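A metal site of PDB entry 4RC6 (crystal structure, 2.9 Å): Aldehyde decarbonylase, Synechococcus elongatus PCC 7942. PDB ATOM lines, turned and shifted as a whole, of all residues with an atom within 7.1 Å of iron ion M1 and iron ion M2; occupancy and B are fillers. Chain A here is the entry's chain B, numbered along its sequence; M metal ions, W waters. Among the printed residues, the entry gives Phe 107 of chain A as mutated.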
ATOM      1  N   VAL A  13       2.757  19.568  20.794  1.00  0.00           N
ATOM      2  CA  VAL A  13       3.370  19.380  19.477  1.00  0.00           C
ATOM      3  C   VAL A  13       3.178  20.636  18.650  1.00  0.00           C
ATOM      4  O   VAL A  13       4.145  21.099  18.050  1.00  0.00           O
ATOM      5  CB  VAL A  13       2.821  18.148  18.688  1.00  0.00           C
ATOM      6  CG1 VAL A  13       3.141  16.852  19.396  1.00  0.00           C
ATOM      7  CG2 VAL A  13       1.351  18.283  18.360  1.00  0.00           C
ATOM      8  N   GLY A  16       5.388  23.073  20.265  1.00  0.00           N
ATOM      9  CA  GLY A  16       6.710  22.593  19.890  1.00  0.00           C
ATOM     10  C   GLY A  16       6.991  22.873  18.426  1.00  0.00           C
ATOM     11  O   GLY A  16       8.091  23.304  18.062  1.00  0.00           O
ATOM     12  N   GLU A  17       5.981  22.663  17.578  1.00  0.00           N
ATOM     13  CA  GLU A  17       6.212  22.842  16.156  1.00  0.00           C
ATOM     14  C   GLU A  17       6.364  24.324  15.864  1.00  0.00           C
ATOM     15  O   GLU A  17       7.169  24.646  15.000  1.00  0.00           O
ATOM     16  CB  GLU A  17       5.110  22.246  15.272  1.00  0.00           C
ATOM     17  CG  GLU A  17       4.967  20.679  15.233  1.00  0.00           C
ATOM     18  CD  GLU A  17       6.073  19.932  14.477  1.00  0.00           C
ATOM     19  OE1 GLU A  17       7.034  20.573  14.002  1.00  0.00           O
ATOM     20  OE2 GLU A  17       6.009  18.677  14.379  1.00  0.00           O
ATOM     21  N   ALA A  20       9.915  25.538  16.976  1.00  0.00           N
ATOM     22  CA  ALA A  20      10.749  24.990  15.934  1.00  0.00           C
ATOM     23  C   ALA A  20      10.660  25.816  14.660  1.00  0.00           C
ATOM     24  O   ALA A  20      11.662  26.011  13.982  1.00  0.00           O
ATOM     25  CB  ALA A  20      10.336  23.572  15.676  1.00  0.00           C
ATOM     26  N   PHE A  21       9.462  26.292  14.317  1.00  0.00           N
ATOM     27  CA  PHE A  21       9.305  27.263  13.207  1.00  0.00           C
ATOM     28  C   PHE A  21      10.143  28.545  13.342  1.00  0.00           C
ATOM     29  O   PHE A  21      11.016  28.781  12.511  1.00  0.00           O
ATOM     30  CB  PHE A  21       7.811  27.605  13.057  1.00  0.00           C
ATOM     31  CG  PHE A  21       7.521  28.932  12.376  1.00  0.00           C
ATOM     32  CD1 PHE A  21       7.702  29.154  11.036  1.00  0.00           C
ATOM     33  CD2 PHE A  21       7.008  29.969  13.143  1.00  0.00           C
ATOM     34  CE1 PHE A  21       7.394  30.422  10.506  1.00  0.00           C
ATOM     35  CE2 PHE A  21       6.686  31.199  12.618  1.00  0.00           C
ATOM     36  CZ  PHE A  21       6.878  31.421  11.304  1.00  0.00           C
ATOM     37  N   TYR A  24      14.094  27.971  13.847  1.00  0.00           N
ATOM     38  CA  TYR A  24      14.893  27.788  12.647  1.00  0.00           C
ATOM     39  C   TYR A  24      14.992  29.133  11.858  1.00  0.00           C
ATOM     40  O   TYR A  24      16.097  29.552  11.491  1.00  0.00           O
ATOM     41  CB  TYR A  24      14.332  26.641  11.788  1.00  0.00           C
ATOM     42  CG  TYR A  24      14.682  25.247  12.292  1.00  0.00           C
ATOM     43  CD1 TYR A  24      16.004  24.841  12.465  1.00  0.00           C
ATOM     44  CD2 TYR A  24      13.685  24.341  12.635  1.00  0.00           C
ATOM     45  CE1 TYR A  24      16.321  23.538  12.945  1.00  0.00           C
ATOM     46  CE2 TYR A  24      13.991  23.064  13.120  1.00  0.00           C
ATOM     47  CZ  TYR A  24      15.311  22.668  13.270  1.00  0.00           C
ATOM     48  OH  TYR A  24      15.578  21.422  13.756  1.00  0.00           O
ATOM     49  N   LEU A  41      13.633  24.240   6.341  1.00  0.00           N
ATOM     50  CA  LEU A  41      13.380  23.559   7.630  1.00  0.00           C
ATOM     51  C   LEU A  41      12.350  24.337   8.440  1.00  0.00           C
ATOM     52  O   LEU A  41      11.385  23.752   8.948  1.00  0.00           O
ATOM     53  CB  LEU A  41      14.652  23.380   8.456  1.00  0.00           C
ATOM     54  CG  LEU A  41      15.829  22.595   7.861  1.00  0.00           C
ATOM     55  CD1 LEU A  41      16.986  22.538   8.855  1.00  0.00           C
ATOM     56  CD2 LEU A  41      15.411  21.200   7.377  1.00  0.00           C
ATOM     57  N   MET A  44       8.704  24.587   6.837  1.00  0.00           N
ATOM     58  CA  MET A  44       8.246  23.237   6.613  1.00  0.00           C
ATOM     59  C   MET A  44       7.452  22.798   7.806  1.00  0.00           C
ATOM     60  O   MET A  44       6.345  22.317   7.694  1.00  0.00           O
ATOM     61  CB  MET A  44       9.434  22.312   6.560  1.00  0.00           C
ATOM     62  CG  MET A  44       9.169  20.853   6.624  1.00  0.00           C
ATOM     63  SD  MET A  44      10.830  20.258   6.326  1.00  0.00           S
ATOM     64  CE  MET A  44      10.548  18.542   6.044  1.00  0.00           C
ATOM     65  N   GLU A  45       8.010  23.072   8.979  1.00  0.00           N
ATOM     66  CA  GLU A  45       7.400  22.736  10.261  1.00  0.00           C
ATOM     67  C   GLU A  45       5.988  23.309  10.376  1.00  0.00           C
ATOM     68  O   GLU A  45       5.138  22.756  11.066  1.00  0.00           O
ATOM     69  CB  GLU A  45       8.277  23.258  11.355  1.00  0.00           C
ATOM     70  CG  GLU A  45       9.571  22.510  11.315  1.00  0.00           C
ATOM     71  CD  GLU A  45      10.036  22.065  12.649  1.00  0.00           C
ATOM     72  OE1 GLU A  45       9.183  21.881  13.541  1.00  0.00           O
ATOM     73  OE2 GLU A  45      11.252  21.850  12.804  1.00  0.00           O
ATOM     74  N   GLN A  46       5.753  24.360   9.626  1.00  0.00           N
ATOM     75  CA  GLN A  46       4.488  25.047   9.509  1.00  0.00           C
ATOM     76  C   GLN A  46       3.364  24.094   9.072  1.00  0.00           C
ATOM     77  O   GLN A  46       2.224  24.171   9.510  1.00  0.00           O
ATOM     78  CB  GLN A  46       4.712  26.117   8.470  1.00  0.00           C
ATOM     79  CG  GLN A  46       3.757  27.272   8.508  1.00  0.00           C
ATOM     80  CD  GLN A  46       2.969  27.410   7.224  1.00  0.00           C
ATOM     81  OE1 GLN A  46       3.174  26.706   6.255  1.00  0.00           O
ATOM     82  NE2 GLN A  46       2.026  28.327   7.224  1.00  0.00           N
ATOM     83  N   HIS A  48       3.556  20.907   9.542  1.00  0.00           N
ATOM     84  CA  HIS A  48       3.456  19.930  10.624  1.00  0.00           C
ATOM     85  C   HIS A  48       2.478  20.526  11.662  1.00  0.00           C
ATOM     86  O   HIS A  48       1.550  19.855  12.124  1.00  0.00           O
ATOM     87  CB  HIS A  48       4.821  19.620  11.274  1.00  0.00           C
ATOM     88  CG  HIS A  48       5.899  19.201  10.326  1.00  0.00           C
ATOM     89  ND1 HIS A  48       6.914  18.339  10.670  1.00  0.00           N
ATOM     90  CD2 HIS A  48       6.168  19.588   9.059  1.00  0.00           C
ATOM     91  CE1 HIS A  48       7.722  18.159   9.649  1.00  0.00           C
ATOM     92  NE2 HIS A  48       7.290  18.917   8.654  1.00  0.00           N
ATOM     93  N   MET A  49       2.720  21.794  11.987  1.00  0.00           N
ATOM     94  CA  MET A  49       1.881  22.593  12.889  1.00  0.00           C
ATOM     95  C   MET A  49       0.418  22.490  12.510  1.00  0.00           C
ATOM     96  O   MET A  49      -0.460  22.100  13.311  1.00  0.00           O
ATOM     97  CB  MET A  49       2.313  24.054  12.828  1.00  0.00           C
ATOM     98  CG  MET A  49       1.570  25.030  13.716  1.00  0.00           C
ATOM     99  SD  MET A  49       2.565  26.529  13.987  1.00  0.00           S
ATOM    100  CE  MET A  49       1.450  27.536  14.970  1.00  0.00           C
ATOM    101  N   PHE A  52      -1.234  18.789  12.824  1.00  0.00           N
ATOM    102  CA  PHE A  52      -1.689  18.233  14.095  1.00  0.00           C
ATOM    103  C   PHE A  52      -2.954  18.884  14.655  1.00  0.00           C
ATOM    104  O   PHE A  52      -3.658  18.272  15.462  1.00  0.00           O
ATOM    105  CB  PHE A  52      -0.544  18.314  15.118  1.00  0.00           C
ATOM    106  CG  PHE A  52       0.617  17.391  14.817  1.00  0.00           C
ATOM    107  CD1 PHE A  52       0.436  15.997  14.817  1.00  0.00           C
ATOM    108  CD2 PHE A  52       1.876  17.907  14.543  1.00  0.00           C
ATOM    109  CE1 PHE A  52       1.492  15.150  14.529  1.00  0.00           C
ATOM    110  CE2 PHE A  52       2.937  17.060  14.268  1.00  0.00           C
ATOM    111  CZ  PHE A  52       2.745  15.685  14.265  1.00  0.00           C
ATOM    112  N   GLN A  95      17.790  23.033  19.577  1.00  0.00           N
ATOM    113  CA  GLN A  95      16.764  22.682  18.597  1.00  0.00           C
ATOM    114  C   GLN A  95      17.030  21.445  17.820  1.00  0.00           C
ATOM    115  O   GLN A  95      16.292  20.499  17.801  1.00  0.00           O
ATOM    116  CB  GLN A  95      16.585  23.797  17.589  1.00  0.00           C
ATOM    117  CG  GLN A  95      15.161  24.266  17.389  1.00  0.00           C
ATOM    118  CD  GLN A  95      14.177  23.148  17.154  1.00  0.00           C
ATOM    119  OE1 GLN A  95      14.293  22.074  17.663  1.00  0.00           O
ATOM    120  NE2 GLN A  95      13.198  23.427  16.358  1.00  0.00           N
ATOM    121  N   ILE A  99      15.392  18.901  20.975  1.00  0.00           N
ATOM    122  CA  ILE A  99      13.966  18.947  20.643  1.00  0.00           C
ATOM    123  C   ILE A  99      13.597  17.953  19.534  1.00  0.00           C
ATOM    124  O   ILE A  99      12.620  17.236  19.657  1.00  0.00           O
ATOM    125  CB  ILE A  99      13.491  20.385  20.242  1.00  0.00           C
ATOM    126  CG1 ILE A  99      13.505  21.337  21.453  1.00  0.00           C
ATOM    127  CG2 ILE A  99      12.069  20.357  19.672  1.00  0.00           C
ATOM    128  CD1 ILE A  99      12.868  22.723  21.207  1.00  0.00           C
ATOM    129  N   GLU A 100      14.355  17.902  18.458  1.00  0.00           N
ATOM    130  CA  GLU A 100      14.004  16.972  17.387  1.00  0.00           C
ATOM    131  C   GLU A 100      14.103  15.506  17.854  1.00  0.00           C
ATOM    132  O   GLU A 100      13.244  14.682  17.473  1.00  0.00           O
ATOM    133  CB  GLU A 100      14.852  17.242  16.141  1.00  0.00           C
ATOM    134  CG  GLU A 100      14.829  18.725  15.675  1.00  0.00           C
ATOM    135  CD  GLU A 100      13.480  19.216  15.057  1.00  0.00           C
ATOM    136  OE1 GLU A 100      12.424  18.543  15.219  1.00  0.00           O
ATOM    137  OE2 GLU A 100      13.475  20.310  14.406  1.00  0.00           O
ATOM    138  N   ALA A 103      10.975  15.083  19.608  1.00  0.00           N
ATOM    139  CA  ALA A 103       9.898  14.848  18.649  1.00  0.00           C
ATOM    140  C   ALA A 103       9.937  13.432  18.090  1.00  0.00           C
ATOM    141  O   ALA A 103       8.921  12.714  18.084  1.00  0.00           O
ATOM    142  CB  ALA A 103       9.966  15.857  17.527  1.00  0.00           C
ATOM    143  N   PHE A 107       6.648  10.688  18.536  1.00  0.00           N
ATOM    144  CA  PHE A 107       5.920  10.213  17.367  1.00  0.00           C
ATOM    145  C   PHE A 107       6.069   8.701  17.175  1.00  0.00           C
ATOM    146  O   PHE A 107       5.076   7.982  16.924  1.00  0.00           O
ATOM    147  CB  PHE A 107       6.386  10.937  16.101  1.00  0.00           C
ATOM    148  CG  PHE A 107       6.359  12.454  16.215  1.00  0.00           C
ATOM    149  CD1 PHE A 107       5.560  13.104  17.175  1.00  0.00           C
ATOM    150  CD2 PHE A 107       7.089  13.243  15.315  1.00  0.00           C
ATOM    151  CE1 PHE A 107       5.547  14.499  17.260  1.00  0.00           C
ATOM    152  CE2 PHE A 107       7.080  14.637  15.375  1.00  0.00           C
ATOM    153  CZ  PHE A 107       6.315  15.270  16.338  1.00  0.00           C
ATOM    154  N   VAL A 125       5.076  13.553   9.011  1.00  0.00           N
ATOM    155  CA  VAL A 125       5.963  14.408   9.807  1.00  0.00           C
ATOM    156  C   VAL A 125       7.274  13.762  10.279  1.00  0.00           C
ATOM    157  O   VAL A 125       8.335  14.400  10.236  1.00  0.00           O
ATOM    158  CB  VAL A 125       5.211  14.959  11.030  1.00  0.00           C
ATOM    159  CG1 VAL A 125       6.172  15.505  12.068  1.00  0.00           C
ATOM    160  CG2 VAL A 125       4.229  16.046  10.606  1.00  0.00           C
ATOM    161  N   ASP A 128      10.667  13.651   8.568  1.00  0.00           N
ATOM    162  CA  ASP A 128      11.223  14.980   8.411  1.00  0.00           C
ATOM    163  C   ASP A 128      12.042  15.459   9.604  1.00  0.00           C
ATOM    164  O   ASP A 128      12.930  16.308   9.486  1.00  0.00           O
ATOM    165  CB  ASP A 128      10.068  15.940   8.138  1.00  0.00           C
ATOM    166  CG  ASP A 128       9.466  15.725   6.748  1.00  0.00           C
ATOM    167  OD1 ASP A 128      10.083  14.991   5.942  1.00  0.00           O
ATOM    168  OD2 ASP A 128       8.389  16.277   6.449  1.00  0.00           O
ATOM    169  N   GLU A 129      11.710  14.930  10.766  1.00  0.00           N
ATOM    170  CA  GLU A 129      12.394  15.321  11.988  1.00  0.00           C
ATOM    171  C   GLU A 129      13.854  14.815  12.052  1.00  0.00           C
ATOM    172  O   GLU A 129      14.732  15.515  12.561  1.00  0.00           O
ATOM    173  CB  GLU A 129      11.557  14.811  13.161  1.00  0.00           C
ATOM    174  CG  GLU A 129      10.084  15.228  13.040  1.00  0.00           C
ATOM    175  CD  GLU A 129       9.823  16.743  13.163  1.00  0.00           C
ATOM    176  OE1 GLU A 129      10.784  17.551  13.237  1.00  0.00           O
ATOM    177  OE2 GLU A 129       8.631  17.142  13.129  1.00  0.00           O
ATOM    178  N   HIS A 132      15.950  17.325  10.320  1.00  0.00           N
ATOM    179  CA  HIS A 132      16.228  18.471  11.185  1.00  0.00           C
ATOM    180  C   HIS A 132      17.428  18.144  12.091  1.00  0.00           C
ATOM    181  O   HIS A 132      18.346  18.962  12.220  1.00  0.00           O
ATOM    182  CB  HIS A 132      14.984  18.845  11.985  1.00  0.00           C
ATOM    183  CG  HIS A 132      13.860  19.344  11.134  1.00  0.00           C
ATOM    184  ND1 HIS A 132      12.541  19.303  11.535  1.00  0.00           N
ATOM    185  CD2 HIS A 132      13.856  19.925   9.908  1.00  0.00           C
ATOM    186  CE1 HIS A 132      11.775  19.814  10.580  1.00  0.00           C
ATOM    187  NE2 HIS A 132      12.552  20.203   9.583  1.00  0.00           N
ATOM    188  N   ARG A 133      17.444  16.937  12.654  1.00  0.00           N
ATOM    189  CA  ARG A 133      18.589  16.447  13.420  1.00  0.00           C
ATOM    190  C   ARG A 133      19.865  16.499  12.557  1.00  0.00           C
ATOM    191  O   ARG A 133      20.951  16.806  13.057  1.00  0.00           O
ATOM    192  CB  ARG A 133      18.328  15.027  13.969  1.00  0.00           C
ATOM    193  CG  ARG A 133      19.622  14.248  14.317  1.00  0.00           C
ATOM    194  CD  ARG A 133      19.529  13.392  15.572  1.00  0.00           C
ATOM    195  NE  ARG A 133      18.847  12.100  15.399  1.00  0.00           N
ATOM    196  CZ  ARG A 133      19.453  10.942  15.134  1.00  0.00           C
ATOM    197  NH1 ARG A 133      20.766  10.876  15.001  1.00  0.00           N
ATOM    198  NH2 ARG A 133      18.734   9.834  15.015  1.00  0.00           N
HETATM  199 FE    FE M   1      11.291  19.846  13.632  1.00  0.00          FE
HETATM  200 FE    FE M   2       8.584  19.538  13.273  1.00  0.00          FE
HETATM  201  O   HOH W   1      10.015  20.142  16.461  1.00  0.00           O
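The side-chain hydroxyl (OH) of Tyr 24 sits close to the side-chain carboxylate (OE2) of Glu 100, at 2.5 Å.
The backbone NH (N) of Glu 100 lies close to the backbone carbonyl oxygen (O) of Gln 95 (3.3 Å).
A ring nitrogen (ND1) of His 48 sits close to the side-chain carboxylate (OE2) of Glu 129 (3.2 Å).
The side-chain sulfur (SD) of Met 44 is in hydrogen-bond range of a ring nitrogen (NE2) of His 132 (3.7 Å).
Within 4 Å of iron ion M1: Glu 45, Glu 100, Glu 129 and His 132.
ND1 of His 48 touches iron ion M2, 3.3 Å away.
The nearest printed residue that does not touch iron ion M2 is His 132 (4.2 Å).
Iron ion M1 is bound by the side-chain carboxylate (OE2) of Glu 45 (2.2 Å), the side-chain carboxylate (OE1) of Glu 100 (2.3 Å), the side-chain carboxylate (OE2) of Glu 100 (2.4 Å), the side-chain carboxylate (OE1) of Glu 129 (2.4 Å) and a ring nitrogen (ND1) of His 132 (2.5 Å).
Iron ion M2 is bound by OE1 of Glu 17 (2.0 Å), OE2 of Glu 129 (2.4 Å) and OE1 of Glu 45 (2.4 Å).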
